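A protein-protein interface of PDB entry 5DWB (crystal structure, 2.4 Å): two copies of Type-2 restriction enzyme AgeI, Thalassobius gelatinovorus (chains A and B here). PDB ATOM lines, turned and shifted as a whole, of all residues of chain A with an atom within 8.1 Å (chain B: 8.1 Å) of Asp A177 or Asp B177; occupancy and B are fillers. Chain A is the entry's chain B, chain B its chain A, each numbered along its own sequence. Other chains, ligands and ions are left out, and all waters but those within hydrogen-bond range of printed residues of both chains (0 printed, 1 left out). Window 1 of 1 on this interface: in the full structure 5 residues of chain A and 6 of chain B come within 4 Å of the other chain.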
ATOM      1  N   VAL A 136     -19.405  32.925  10.912  1.00  0.00           N
ATOM      2  CA  VAL A 136     -19.276  32.721  12.356  1.00  0.00           C
ATOM      3  C   VAL A 136     -19.087  34.050  13.095  1.00  0.00           C
ATOM      4  O   VAL A 136     -18.501  34.992  12.557  1.00  0.00           O
ATOM      5  CB  VAL A 136     -18.075  31.770  12.669  1.00  0.00           C
ATOM      6  CG1 VAL A 136     -17.847  31.603  14.170  1.00  0.00           C
ATOM      7  CG2 VAL A 136     -18.273  30.414  12.014  1.00  0.00           C
ATOM      8  N   GLY A 137     -19.574  34.115  14.333  1.00  0.00           N
ATOM      9  CA  GLY A 137     -19.450  35.301  15.164  1.00  0.00           C
ATOM     10  C   GLY A 137     -18.011  35.675  15.474  1.00  0.00           C
ATOM     11  O   GLY A 137     -17.130  34.818  15.457  1.00  0.00           O
ATOM     12  N   LYS A 140     -16.332  33.525  18.619  1.00  0.00           N
ATOM     13  CA  LYS A 140     -16.850  32.185  18.876  1.00  0.00           C
ATOM     14  C   LYS A 140     -15.799  31.073  18.861  1.00  0.00           C
ATOM     15  O   LYS A 140     -16.077  29.961  18.406  1.00  0.00           O
ATOM     16  CB  LYS A 140     -17.962  31.849  17.881  1.00  0.00           C
ATOM     17  CG  LYS A 140     -19.312  31.660  18.558  1.00  0.00           C
ATOM     18  CD  LYS A 140     -19.185  30.681  19.717  1.00  0.00           C
ATOM     19  CE  LYS A 140     -20.181  30.982  20.819  1.00  0.00           C
ATOM     20  NZ  LYS A 140     -19.846  30.250  22.075  1.00  0.00           N
ATOM     21  N   HIS A 166     -13.468  24.796  21.939  1.00  0.00           N
ATOM     22  CA  HIS A 166     -14.538  25.475  22.652  1.00  0.00           C
ATOM     23  C   HIS A 166     -14.436  25.058  24.109  1.00  0.00           C
ATOM     24  O   HIS A 166     -14.677  23.899  24.442  1.00  0.00           O
ATOM     25  CB  HIS A 166     -15.908  25.113  22.069  1.00  0.00           C
ATOM     26  CG  HIS A 166     -16.032  25.380  20.596  1.00  0.00           C
ATOM     27  ND1 HIS A 166     -16.400  26.602  20.091  1.00  0.00           N
ATOM     28  CD2 HIS A 166     -15.818  24.572  19.529  1.00  0.00           C
ATOM     29  CE1 HIS A 166     -16.424  26.539  18.764  1.00  0.00           C
ATOM     30  NE2 HIS A 166     -16.077  25.319  18.404  1.00  0.00           N
ATOM     31  N   LYS A 168     -15.416  25.185  28.055  1.00  0.00           N
ATOM     32  CA  LYS A 168     -16.486  25.488  28.999  1.00  0.00           C
ATOM     33  C   LYS A 168     -16.239  24.764  30.309  1.00  0.00           C
ATOM     34  O   LYS A 168     -16.118  23.541  30.332  1.00  0.00           O
ATOM     35  CB  LYS A 168     -17.861  25.087  28.448  1.00  0.00           C
ATOM     36  CG  LYS A 168     -18.132  25.536  27.028  1.00  0.00           C
ATOM     37  CD  LYS A 168     -19.613  25.558  26.712  1.00  0.00           C
ATOM     38  CE  LYS A 168     -20.195  26.921  27.039  1.00  0.00           C
ATOM     39  NZ  LYS A 168     -19.562  27.992  26.201  1.00  0.00           N
ATOM     40  N   LEU A 171     -21.583  23.336  31.229  1.00  0.00           N
ATOM     41  CA  LEU A 171     -22.370  23.382  29.999  1.00  0.00           C
ATOM     42  C   LEU A 171     -23.655  24.195  30.098  1.00  0.00           C
ATOM     43  O   LEU A 171     -23.849  25.143  29.335  1.00  0.00           O
ATOM     44  CB  LEU A 171     -22.724  21.963  29.547  1.00  0.00           C
ATOM     45  CG  LEU A 171     -21.551  20.997  29.413  1.00  0.00           C
ATOM     46  CD1 LEU A 171     -22.031  19.638  28.943  1.00  0.00           C
ATOM     47  CD2 LEU A 171     -20.524  21.572  28.453  1.00  0.00           C
ATOM     48  N   ALA A 172     -24.536  23.797  31.015  1.00  0.00           N
ATOM     49  CA  ALA A 172     -25.881  24.362  31.107  1.00  0.00           C
ATOM     50  C   ALA A 172     -26.522  24.388  29.716  1.00  0.00           C
ATOM     51  O   ALA A 172     -26.410  23.427  28.949  1.00  0.00           O
ATOM     52  CB  ALA A 172     -25.849  25.754  31.723  1.00  0.00           C
ATOM     53  N   GLU A 173     -27.127  25.517  29.371  1.00  0.00           N
ATOM     54  CA  GLU A 173     -27.696  25.696  28.046  1.00  0.00           C
ATOM     55  C   GLU A 173     -26.709  26.457  27.167  1.00  0.00           C
ATOM     56  O   GLU A 173     -26.927  26.648  25.967  1.00  0.00           O
ATOM     57  CB  GLU A 173     -29.026  26.445  28.135  1.00  0.00           C
ATOM     58  CG  GLU A 173     -28.897  27.974  28.225  1.00  0.00           C
ATOM     59  CD  GLU A 173     -28.389  28.484  29.577  1.00  0.00           C
ATOM     60  OE1 GLU A 173     -28.190  27.674  30.514  1.00  0.00           O
ATOM     61  OE2 GLU A 173     -28.203  29.717  29.704  1.00  0.00           O
ATOM     62  N   ARG A 174     -25.595  26.844  27.773  1.00  0.00           N
ATOM     63  CA  ARG A 174     -24.622  27.721  27.133  1.00  0.00           C
ATOM     64  C   ARG A 174     -23.823  27.006  26.054  1.00  0.00           C
ATOM     65  O   ARG A 174     -23.274  27.637  25.164  1.00  0.00           O
ATOM     66  CB  ARG A 174     -23.689  28.293  28.194  1.00  0.00           C
ATOM     67  CG  ARG A 174     -24.403  29.227  29.150  1.00  0.00           C
ATOM     68  CD  ARG A 174     -23.531  29.638  30.312  1.00  0.00           C
ATOM     69  NE  ARG A 174     -23.465  28.639  31.370  1.00  0.00           N
ATOM     70  CZ  ARG A 174     -22.474  27.772  31.542  1.00  0.00           C
ATOM     71  NH1 ARG A 174     -21.436  27.755  30.712  1.00  0.00           N
ATOM     72  NH2 ARG A 174     -22.527  26.911  32.554  1.00  0.00           N
ATOM     73  N   VAL A 175     -23.790  25.682  26.127  1.00  0.00           N
ATOM     74  CA  VAL A 175     -23.110  24.863  25.137  1.00  0.00           C
ATOM     75  C   VAL A 175     -23.735  25.061  23.739  1.00  0.00           C
ATOM     76  O   VAL A 175     -23.063  24.901  22.719  1.00  0.00           O
ATOM     77  CB  VAL A 175     -23.143  23.366  25.558  1.00  0.00           C
ATOM     78  CG1 VAL A 175     -24.572  22.918  25.828  1.00  0.00           C
ATOM     79  CG2 VAL A 175     -22.491  22.476  24.509  1.00  0.00           C
ATOM     80  N   SER A 176     -25.012  25.446  23.691  1.00  0.00           N
ATOM     81  CA  SER A 176     -25.690  25.706  22.418  1.00  0.00           C
ATOM     82  C   SER A 176     -25.134  26.926  21.672  1.00  0.00           C
ATOM     83  O   SER A 176     -25.411  27.110  20.489  1.00  0.00           O
ATOM     84  CB  SER A 176     -27.195  25.889  22.636  1.00  0.00           C
ATOM     85  OG  SER A 176     -27.771  24.741  23.230  1.00  0.00           O
ATOM     86  N   ASP A 177     -24.381  27.768  22.370  1.00  0.00           N
ATOM     87  CA  ASP A 177     -23.684  28.887  21.737  1.00  0.00           C
ATOM     88  C   ASP A 177     -22.705  28.390  20.692  1.00  0.00           C
ATOM     89  O   ASP A 177     -22.590  28.950  19.606  1.00  0.00           O
ATOM     90  CB  ASP A 177     -22.931  29.723  22.776  1.00  0.00           C
ATOM     91  CG  ASP A 177     -23.854  30.508  23.679  1.00  0.00           C
ATOM     92  OD1 ASP A 177     -25.037  30.668  23.317  1.00  0.00           O
ATOM     93  OD2 ASP A 177     -23.399  30.956  24.758  1.00  0.00           O
ATOM     94  N   ASP A 178     -22.000  27.322  21.041  1.00  0.00           N
ATOM     95  CA  ASP A 178     -20.845  26.869  20.285  1.00  0.00           C
ATOM     96  C   ASP A 178     -21.199  25.991  19.096  1.00  0.00           C
ATOM     97  O   ASP A 178     -20.427  25.892  18.144  1.00  0.00           O
ATOM     98  CB  ASP A 178     -19.907  26.111  21.221  1.00  0.00           C
ATOM     99  CG  ASP A 178     -19.657  26.861  22.512  1.00  0.00           C
ATOM    100  OD1 ASP A 178     -19.493  28.094  22.444  1.00  0.00           O
ATOM    101  OD2 ASP A 178     -19.657  26.232  23.593  1.00  0.00           O
ATOM    102  N   ILE A 179     -22.368  25.361  19.157  1.00  0.00           N
ATOM    103  CA  ILE A 179     -22.743  24.347  18.175  1.00  0.00           C
ATOM    104  C   ILE A 179     -22.818  24.862  16.725  1.00  0.00           C
ATOM    105  O   ILE A 179     -22.295  24.205  15.822  1.00  0.00           O
ATOM    106  CB  ILE A 179     -24.070  23.685  18.566  1.00  0.00           C
ATOM    107  CG1 ILE A 179     -23.849  22.802  19.798  1.00  0.00           C
ATOM    108  CG2 ILE A 179     -24.632  22.880  17.403  1.00  0.00           C
ATOM    109  CD1 ILE A 179     -25.116  22.341  20.477  1.00  0.00           C
ATOM    110  N   PRO A 180     -23.451  26.030  16.486  1.00  0.00           N
ATOM    111  CA  PRO A 180     -23.446  26.503  15.094  1.00  0.00           C
ATOM    112  C   PRO A 180     -22.041  26.789  14.578  1.00  0.00           C
ATOM    113  O   PRO A 180     -21.696  26.363  13.476  1.00  0.00           O
ATOM    114  CB  PRO A 180     -24.263  27.797  15.154  1.00  0.00           C
ATOM    115  CG  PRO A 180     -25.078  27.677  16.385  1.00  0.00           C
ATOM    116  CD  PRO A 180     -24.248  26.909  17.358  1.00  0.00           C
ATOM    117  N   ALA A 181     -21.242  27.497  15.373  1.00  0.00           N
ATOM    118  CA  ALA A 181     -19.855  27.794  15.011  1.00  0.00           C
ATOM    119  C   ALA A 181     -19.053  26.515  14.827  1.00  0.00           C
ATOM    120  O   ALA A 181     -18.262  26.393  13.886  1.00  0.00           O
ATOM    121  CB  ALA A 181     -19.203  28.678  16.062  1.00  0.00           C
ATOM    122  N   SER A 182     -19.270  25.563  15.727  1.00  0.00           N
ATOM    123  CA  SER A 182     -18.548  24.305  15.691  1.00  0.00           C
ATOM    124  C   SER A 182     -18.840  23.550  14.401  1.00  0.00           C
ATOM    125  O   SER A 182     -17.932  23.005  13.771  1.00  0.00           O
ATOM    126  CB  SER A 182     -18.910  23.450  16.902  1.00  0.00           C
ATOM    127  OG  SER A 182     -18.179  22.238  16.906  1.00  0.00           O
ATOM    128  N   TYR A 227     -25.626  15.981  21.706  1.00  0.00           N
ATOM    129  CA  TYR A 227     -24.939  17.030  20.959  1.00  0.00           C
ATOM    130  C   TYR A 227     -23.681  16.448  20.323  1.00  0.00           C
ATOM    131  O   TYR A 227     -23.326  16.776  19.196  1.00  0.00           O
ATOM    132  CB  TYR A 227     -24.573  18.208  21.861  1.00  0.00           C
ATOM    133  CG  TYR A 227     -25.731  19.102  22.269  1.00  0.00           C
ATOM    134  CD1 TYR A 227     -26.845  19.263  21.453  1.00  0.00           C
ATOM    135  CD2 TYR A 227     -25.695  19.798  23.473  1.00  0.00           C
ATOM    136  CE1 TYR A 227     -27.894  20.084  21.832  1.00  0.00           C
ATOM    137  CE2 TYR A 227     -26.739  20.618  23.859  1.00  0.00           C
ATOM    138  CZ  TYR A 227     -27.833  20.756  23.035  1.00  0.00           C
ATOM    139  OH  TYR A 227     -28.863  21.578  23.428  1.00  0.00           O
ATOM    140  N   PHE A 234     -19.544  18.400  17.594  1.00  0.00           N
ATOM    141  CA  PHE A 234     -18.137  18.655  17.867  1.00  0.00           C
ATOM    142  C   PHE A 234     -17.305  17.463  17.395  1.00  0.00           C
ATOM    143  O   PHE A 234     -17.802  16.333  17.379  1.00  0.00           O
ATOM    144  CB  PHE A 234     -17.901  18.909  19.358  1.00  0.00           C
ATOM    145  CG  PHE A 234     -18.650  20.094  19.905  1.00  0.00           C
ATOM    146  CD1 PHE A 234     -18.094  21.360  19.874  1.00  0.00           C
ATOM    147  CD2 PHE A 234     -19.905  19.936  20.477  1.00  0.00           C
ATOM    148  CE1 PHE A 234     -18.781  22.450  20.387  1.00  0.00           C
ATOM    149  CE2 PHE A 234     -20.595  21.017  20.994  1.00  0.00           C
ATOM    150  CZ  PHE A 234     -20.032  22.276  20.951  1.00  0.00           C
ATOM    151  N   GLY B 137     -33.978  22.063  19.034  1.00  0.00           N
ATOM    152  CA  GLY B 137     -33.808  21.577  20.393  1.00  0.00           C
ATOM    153  C   GLY B 137     -35.113  21.508  21.165  1.00  0.00           C
ATOM    154  O   GLY B 137     -36.068  22.217  20.855  1.00  0.00           O
ATOM    155  N   LYS B 140     -36.459  25.121  23.014  1.00  0.00           N
ATOM    156  CA  LYS B 140     -35.996  26.363  22.400  1.00  0.00           C
ATOM    157  C   LYS B 140     -37.096  27.350  21.984  1.00  0.00           C
ATOM    158  O   LYS B 140     -36.971  28.029  20.964  1.00  0.00           O
ATOM    159  CB  LYS B 140     -35.135  26.024  21.180  1.00  0.00           C
ATOM    160  N   HIS B 166     -39.101  34.356  21.510  1.00  0.00           N
ATOM    161  CA  HIS B 166     -37.893  34.097  22.273  1.00  0.00           C
ATOM    162  C   HIS B 166     -37.686  35.270  23.222  1.00  0.00           C
ATOM    163  O   HIS B 166     -37.398  36.382  22.784  1.00  0.00           O
ATOM    164  CB  HIS B 166     -36.694  33.900  21.343  1.00  0.00           C
ATOM    165  CG  HIS B 166     -36.915  32.853  20.301  1.00  0.00           C
ATOM    166  ND1 HIS B 166     -36.698  31.503  20.535  1.00  0.00           N
ATOM    167  CD2 HIS B 166     -37.347  32.935  19.022  1.00  0.00           C
ATOM    168  CE1 HIS B 166     -36.980  30.819  19.451  1.00  0.00           C
ATOM    169  NE2 HIS B 166     -37.382  31.666  18.507  1.00  0.00           N
ATOM    170  N   LYS B 168     -35.908  37.348  26.276  1.00  0.00           N
ATOM    171  CA  LYS B 168     -34.658  37.577  27.002  1.00  0.00           C
ATOM    172  C   LYS B 168     -34.720  38.932  27.682  1.00  0.00           C
ATOM    173  O   LYS B 168     -34.883  39.948  27.016  1.00  0.00           O
ATOM    174  CB  LYS B 168     -33.434  37.518  26.066  1.00  0.00           C
ATOM    175  CG  LYS B 168     -33.387  36.306  25.143  1.00  0.00           C
ATOM    176  CD  LYS B 168     -31.992  36.061  24.582  1.00  0.00           C
ATOM    177  CE  LYS B 168     -31.176  35.139  25.474  1.00  0.00           C
ATOM    178  NZ  LYS B 168     -31.762  33.774  25.596  1.00  0.00           N
ATOM    179  N   LEU B 171     -29.429  40.474  26.693  1.00  0.00           N
ATOM    180  CA  LEU B 171     -28.883  39.674  25.601  1.00  0.00           C
ATOM    181  C   LEU B 171     -27.546  39.015  25.894  1.00  0.00           C
ATOM    182  O   LEU B 171     -27.431  37.792  25.820  1.00  0.00           O
ATOM    183  CB  LEU B 171     -28.748  40.533  24.354  1.00  0.00           C
ATOM    184  CG  LEU B 171     -30.013  41.289  23.978  1.00  0.00           C
ATOM    185  CD1 LEU B 171     -29.752  42.075  22.707  1.00  0.00           C
ATOM    186  CD2 LEU B 171     -31.177  40.325  23.819  1.00  0.00           C
ATOM    187  N   ALA B 172     -26.537  39.832  26.195  1.00  0.00           N
ATOM    188  CA  ALA B 172     -25.155  39.359  26.336  1.00  0.00           C
ATOM    189  C   ALA B 172     -24.755  38.483  25.144  1.00  0.00           C
ATOM    190  O   ALA B 172     -24.968  38.857  23.991  1.00  0.00           O
ATOM    191  CB  ALA B 172     -24.971  38.614  27.642  1.00  0.00           C
ATOM    192  N   GLU B 173     -24.180  37.318  25.421  1.00  0.00           N
ATOM    193  CA  GLU B 173     -23.851  36.383  24.353  1.00  0.00           C
ATOM    194  C   GLU B 173     -24.931  35.313  24.240  1.00  0.00           C
ATOM    195  O   GLU B 173     -24.876  34.442  23.370  1.00  0.00           O
ATOM    196  CB  GLU B 173     -22.497  35.725  24.603  1.00  0.00           C
ATOM    197  CG  GLU B 173     -22.549  34.498  25.517  1.00  0.00           C
ATOM    198  CD  GLU B 173     -22.794  34.832  26.975  1.00  0.00           C
ATOM    199  OE1 GLU B 173     -22.860  36.032  27.321  1.00  0.00           O
ATOM    200  OE2 GLU B 173     -22.906  33.882  27.782  1.00  0.00           O
ATOM    201  N   ARG B 174     -25.908  35.393  25.137  1.00  0.00           N
ATOM    202  CA  ARG B 174     -26.942  34.372  25.293  1.00  0.00           C
ATOM    203  C   ARG B 174     -28.003  34.423  24.197  1.00  0.00           C
ATOM    204  O   ARG B 174     -28.726  33.458  23.979  1.00  0.00           O
ATOM    205  CB  ARG B 174     -27.590  34.517  26.672  1.00  0.00           C
ATOM    206  CG  ARG B 174     -26.630  34.216  27.805  1.00  0.00           C
ATOM    207  CD  ARG B 174     -27.202  34.567  29.172  1.00  0.00           C
ATOM    208  NE  ARG B 174     -27.154  36.005  29.424  1.00  0.00           N
ATOM    209  CZ  ARG B 174     -28.196  36.821  29.303  1.00  0.00           C
ATOM    210  NH1 ARG B 174     -29.387  36.336  28.982  1.00  0.00           N
ATOM    211  NH2 ARG B 174     -28.054  38.116  29.541  1.00  0.00           N
ATOM    212  N   VAL B 175     -28.097  35.558  23.513  1.00  0.00           N
ATOM    213  CA  VAL B 175     -29.052  35.721  22.425  1.00  0.00           C
ATOM    214  C   VAL B 175     -28.772  34.692  21.311  1.00  0.00           C
ATOM    215  O   VAL B 175     -29.672  34.310  20.563  1.00  0.00           O
ATOM    216  CB  VAL B 175     -29.024  37.176  21.881  1.00  0.00           C
ATOM    217  CG1 VAL B 175     -27.603  37.592  21.528  1.00  0.00           C
ATOM    218  CG2 VAL B 175     -29.977  37.347  20.690  1.00  0.00           C
ATOM    219  N   SER B 176     -27.527  34.230  21.223  1.00  0.00           N
ATOM    220  CA  SER B 176     -27.147  33.198  20.257  1.00  0.00           C
ATOM    221  C   SER B 176     -27.768  31.829  20.541  1.00  0.00           C
ATOM    222  O   SER B 176     -27.756  30.952  19.674  1.00  0.00           O
ATOM    223  CB  SER B 176     -25.627  33.055  20.202  1.00  0.00           C
ATOM    224  OG  SER B 176     -25.022  34.276  19.833  1.00  0.00           O
ATOM    225  N   ASP B 177     -28.315  31.645  21.740  1.00  0.00           N
ATOM    226  CA  ASP B 177     -28.990  30.390  22.082  1.00  0.00           C
ATOM    227  C   ASP B 177     -30.115  30.095  21.107  1.00  0.00           C
ATOM    228  O   ASP B 177     -30.291  28.972  20.641  1.00  0.00           O
ATOM    229  CB  ASP B 177     -29.598  30.457  23.486  1.00  0.00           C
ATOM    230  CG  ASP B 177     -28.562  30.532  24.575  1.00  0.00           C
ATOM    231  OD1 ASP B 177     -27.378  30.246  24.295  1.00  0.00           O
ATOM    232  OD2 ASP B 177     -28.939  30.885  25.720  1.00  0.00           O
ATOM    233  N   ASP B 178     -30.876  31.135  20.811  1.00  0.00           N
ATOM    234  CA  ASP B 178     -32.148  30.998  20.128  1.00  0.00           C
ATOM    235  C   ASP B 178     -32.036  30.974  18.611  1.00  0.00           C
ATOM    236  O   ASP B 178     -32.952  30.515  17.932  1.00  0.00           O
ATOM    237  CB  ASP B 178     -33.077  32.121  20.587  1.00  0.00           C
ATOM    238  CG  ASP B 178     -33.091  32.270  22.102  1.00  0.00           C
ATOM    239  OD1 ASP B 178     -33.074  31.234  22.804  1.00  0.00           O
ATOM    240  OD2 ASP B 178     -33.105  33.418  22.594  1.00  0.00           O
ATOM    241  N   ILE B 179     -30.919  31.468  18.083  1.00  0.00           N
ATOM    242  CA  ILE B 179     -30.785  31.699  16.642  1.00  0.00           C
ATOM    243  C   ILE B 179     -30.989  30.459  15.745  1.00  0.00           C
ATOM    244  O   ILE B 179     -31.703  30.552  14.746  1.00  0.00           O
ATOM    245  CB  ILE B 179     -29.411  32.338  16.322  1.00  0.00           C
ATOM    246  CG1 ILE B 179     -29.388  33.789  16.807  1.00  0.00           C
ATOM    247  CG2 ILE B 179     -29.106  32.282  14.831  1.00  0.00           C
ATOM    248  CD1 ILE B 179     -28.005  34.408  16.841  1.00  0.00           C
ATOM    249  N   PRO B 180     -30.393  29.300  16.088  1.00  0.00           N
ATOM    250  CA  PRO B 180     -30.651  28.159  15.192  1.00  0.00           C
ATOM    251  C   PRO B 180     -32.132  27.768  15.133  1.00  0.00           C
ATOM    252  O   PRO B 180     -32.690  27.596  14.045  1.00  0.00           O
ATOM    253  CB  PRO B 180     -29.827  27.024  15.812  1.00  0.00           C
ATOM    254  CG  PRO B 180     -28.799  27.705  16.655  1.00  0.00           C
ATOM    255  CD  PRO B 180     -29.454  28.947  17.170  1.00  0.00           C
ATOM    256  N   ALA B 181     -32.759  27.654  16.299  1.00  0.00           N
ATOM    257  CA  ALA B 181     -34.183  27.344  16.379  1.00  0.00           C
ATOM    258  C   ALA B 181     -35.018  28.397  15.658  1.00  0.00           C
ATOM    259  O   ALA B 181     -35.990  28.073  14.972  1.00  0.00           O
ATOM    260  CB  ALA B 181     -34.618  27.226  17.828  1.00  0.00           C
ATOM    261  N   SER B 182     -34.643  29.659  15.825  1.00  0.00           N
ATOM    262  CA  SER B 182     -35.381  30.751  15.216  1.00  0.00           C
ATOM    263  C   SER B 182     -35.370  30.676  13.692  1.00  0.00           C
ATOM    264  O   SER B 182     -36.408  30.847  13.048  1.00  0.00           O
ATOM    265  CB  SER B 182     -34.806  32.093  15.676  1.00  0.00           C
ATOM    266  OG  SER B 182     -35.526  33.180  15.119  1.00  0.00           O
ATOM    267  N   TYR B 227     -27.590  40.658  14.101  1.00  0.00           N
ATOM    268  CA  TYR B 227     -28.354  39.419  14.226  1.00  0.00           C
ATOM    269  C   TYR B 227     -29.715  39.604  13.568  1.00  0.00           C
ATOM    270  O   TYR B 227     -30.229  38.706  12.895  1.00  0.00           O
ATOM    271  CB  TYR B 227     -28.536  39.021  15.696  1.00  0.00           C
ATOM    272  CG  TYR B 227     -27.320  38.421  16.365  1.00  0.00           C
ATOM    273  CD1 TYR B 227     -26.396  37.672  15.644  1.00  0.00           C
ATOM    274  CD2 TYR B 227     -27.087  38.624  17.717  1.00  0.00           C
ATOM    275  CE1 TYR B 227     -25.281  37.124  16.264  1.00  0.00           C
ATOM    276  CE2 TYR B 227     -25.976  38.088  18.342  1.00  0.00           C
ATOM    277  CZ  TYR B 227     -25.078  37.340  17.616  1.00  0.00           C
ATOM    278  OH  TYR B 227     -23.976  36.813  18.251  1.00  0.00           O
ATOM    279  N   PHE B 234     -34.224  36.750  13.293  1.00  0.00           N
ATOM    280  CA  PHE B 234     -35.543  36.809  13.906  1.00  0.00           C
ATOM    281  C   PHE B 234     -36.491  37.568  12.991  1.00  0.00           C
ATOM    282  O   PHE B 234     -36.060  38.430  12.226  1.00  0.00           O
ATOM    283  CB  PHE B 234     -35.473  37.475  15.286  1.00  0.00           C
ATOM    284  CG  PHE B 234     -34.600  36.746  16.269  1.00  0.00           C
ATOM    285  CD1 PHE B 234     -35.129  35.757  17.087  1.00  0.00           C
ATOM    286  CD2 PHE B 234     -33.244  37.043  16.367  1.00  0.00           C
ATOM    287  CE1 PHE B 234     -34.326  35.081  17.995  1.00  0.00           C
ATOM    288  CE2 PHE B 234     -32.436  36.369  17.271  1.00  0.00           C
ATOM    289  CZ  PHE B 234     -32.982  35.385  18.088  1.00  0.00           C
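OD1 of Asp B177 sits close to OD1 of Asp A177.
The side-chain hydroxyl of Ser A176 lies close to the backbone carbonyl oxygen of Glu A173 (3.4 Å).
OG of Ser B176 is in hydrogen-bond range of OH of Tyr B227 (3.2 Å).
Among the printed residues, pairs that only touch across the chains: Glu A173 with Asp B177 (3.8 Å), Asp A177 with Glu B173 (3.7 Å), Asp A177 with Ser B176 (3.97 Å) and Pro A180 with Pro B180 (3.7 Å).
Asp A177 touches just these residues of chain B: Glu B173, Ser B176 and Asp B177.
Asp B177 touches two residues of chain A.
Of the printed residues of chain B, Glu A173 touches Asp B177 (3.8 Å).
Of the printed residues of chain A, Pro B180 touches Pro A180 (3.7 Å).
Of the printed residues of chain B, Pro A180 touches Pro B180.
Lys A168 touches none of the printed residues of chain B.
Tyr A227 touches none of the printed residues of chain B.
The nearest printed residue of chain B that does not touch Pro A180 is Ser B176 (5.4 Å).
Of the 19 printed residues of chain A, 3 touch a printed residue of chain B.
Hydrophobic or aromatic side chains of chain A within 4 Å of the printed part of chain B: Pro A180.
Along chain A the printed residues that touch a printed residue of chain B span positions 173 to 180.
Printed residues of chain B that touch a printed residue of chain A: Glu B173, Ser B176, Asp B177 and Pro B180.
Among the printed residues, no Asp or Glu carboxylate lies within 4 Å of a Lys or Arg side-chain nitrogen of the other chain.
Glu A173 touches Asp B177, and with the chains exchanged Asp A177 touches Glu B173.
Asp A177 touches Ser B176, but with the chains exchanged Ser A176 does not touch Asp B177 (4.7 Å).
Asp B177 touches its own counterpart, Asp A177.
Pro A180 touches its own counterpart, Pro B180.
18 positions are printed for both chains.
Of the 5 pairs that touch across the chains among the printed residues, 4 have their exchanged pair printed and touching as well.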
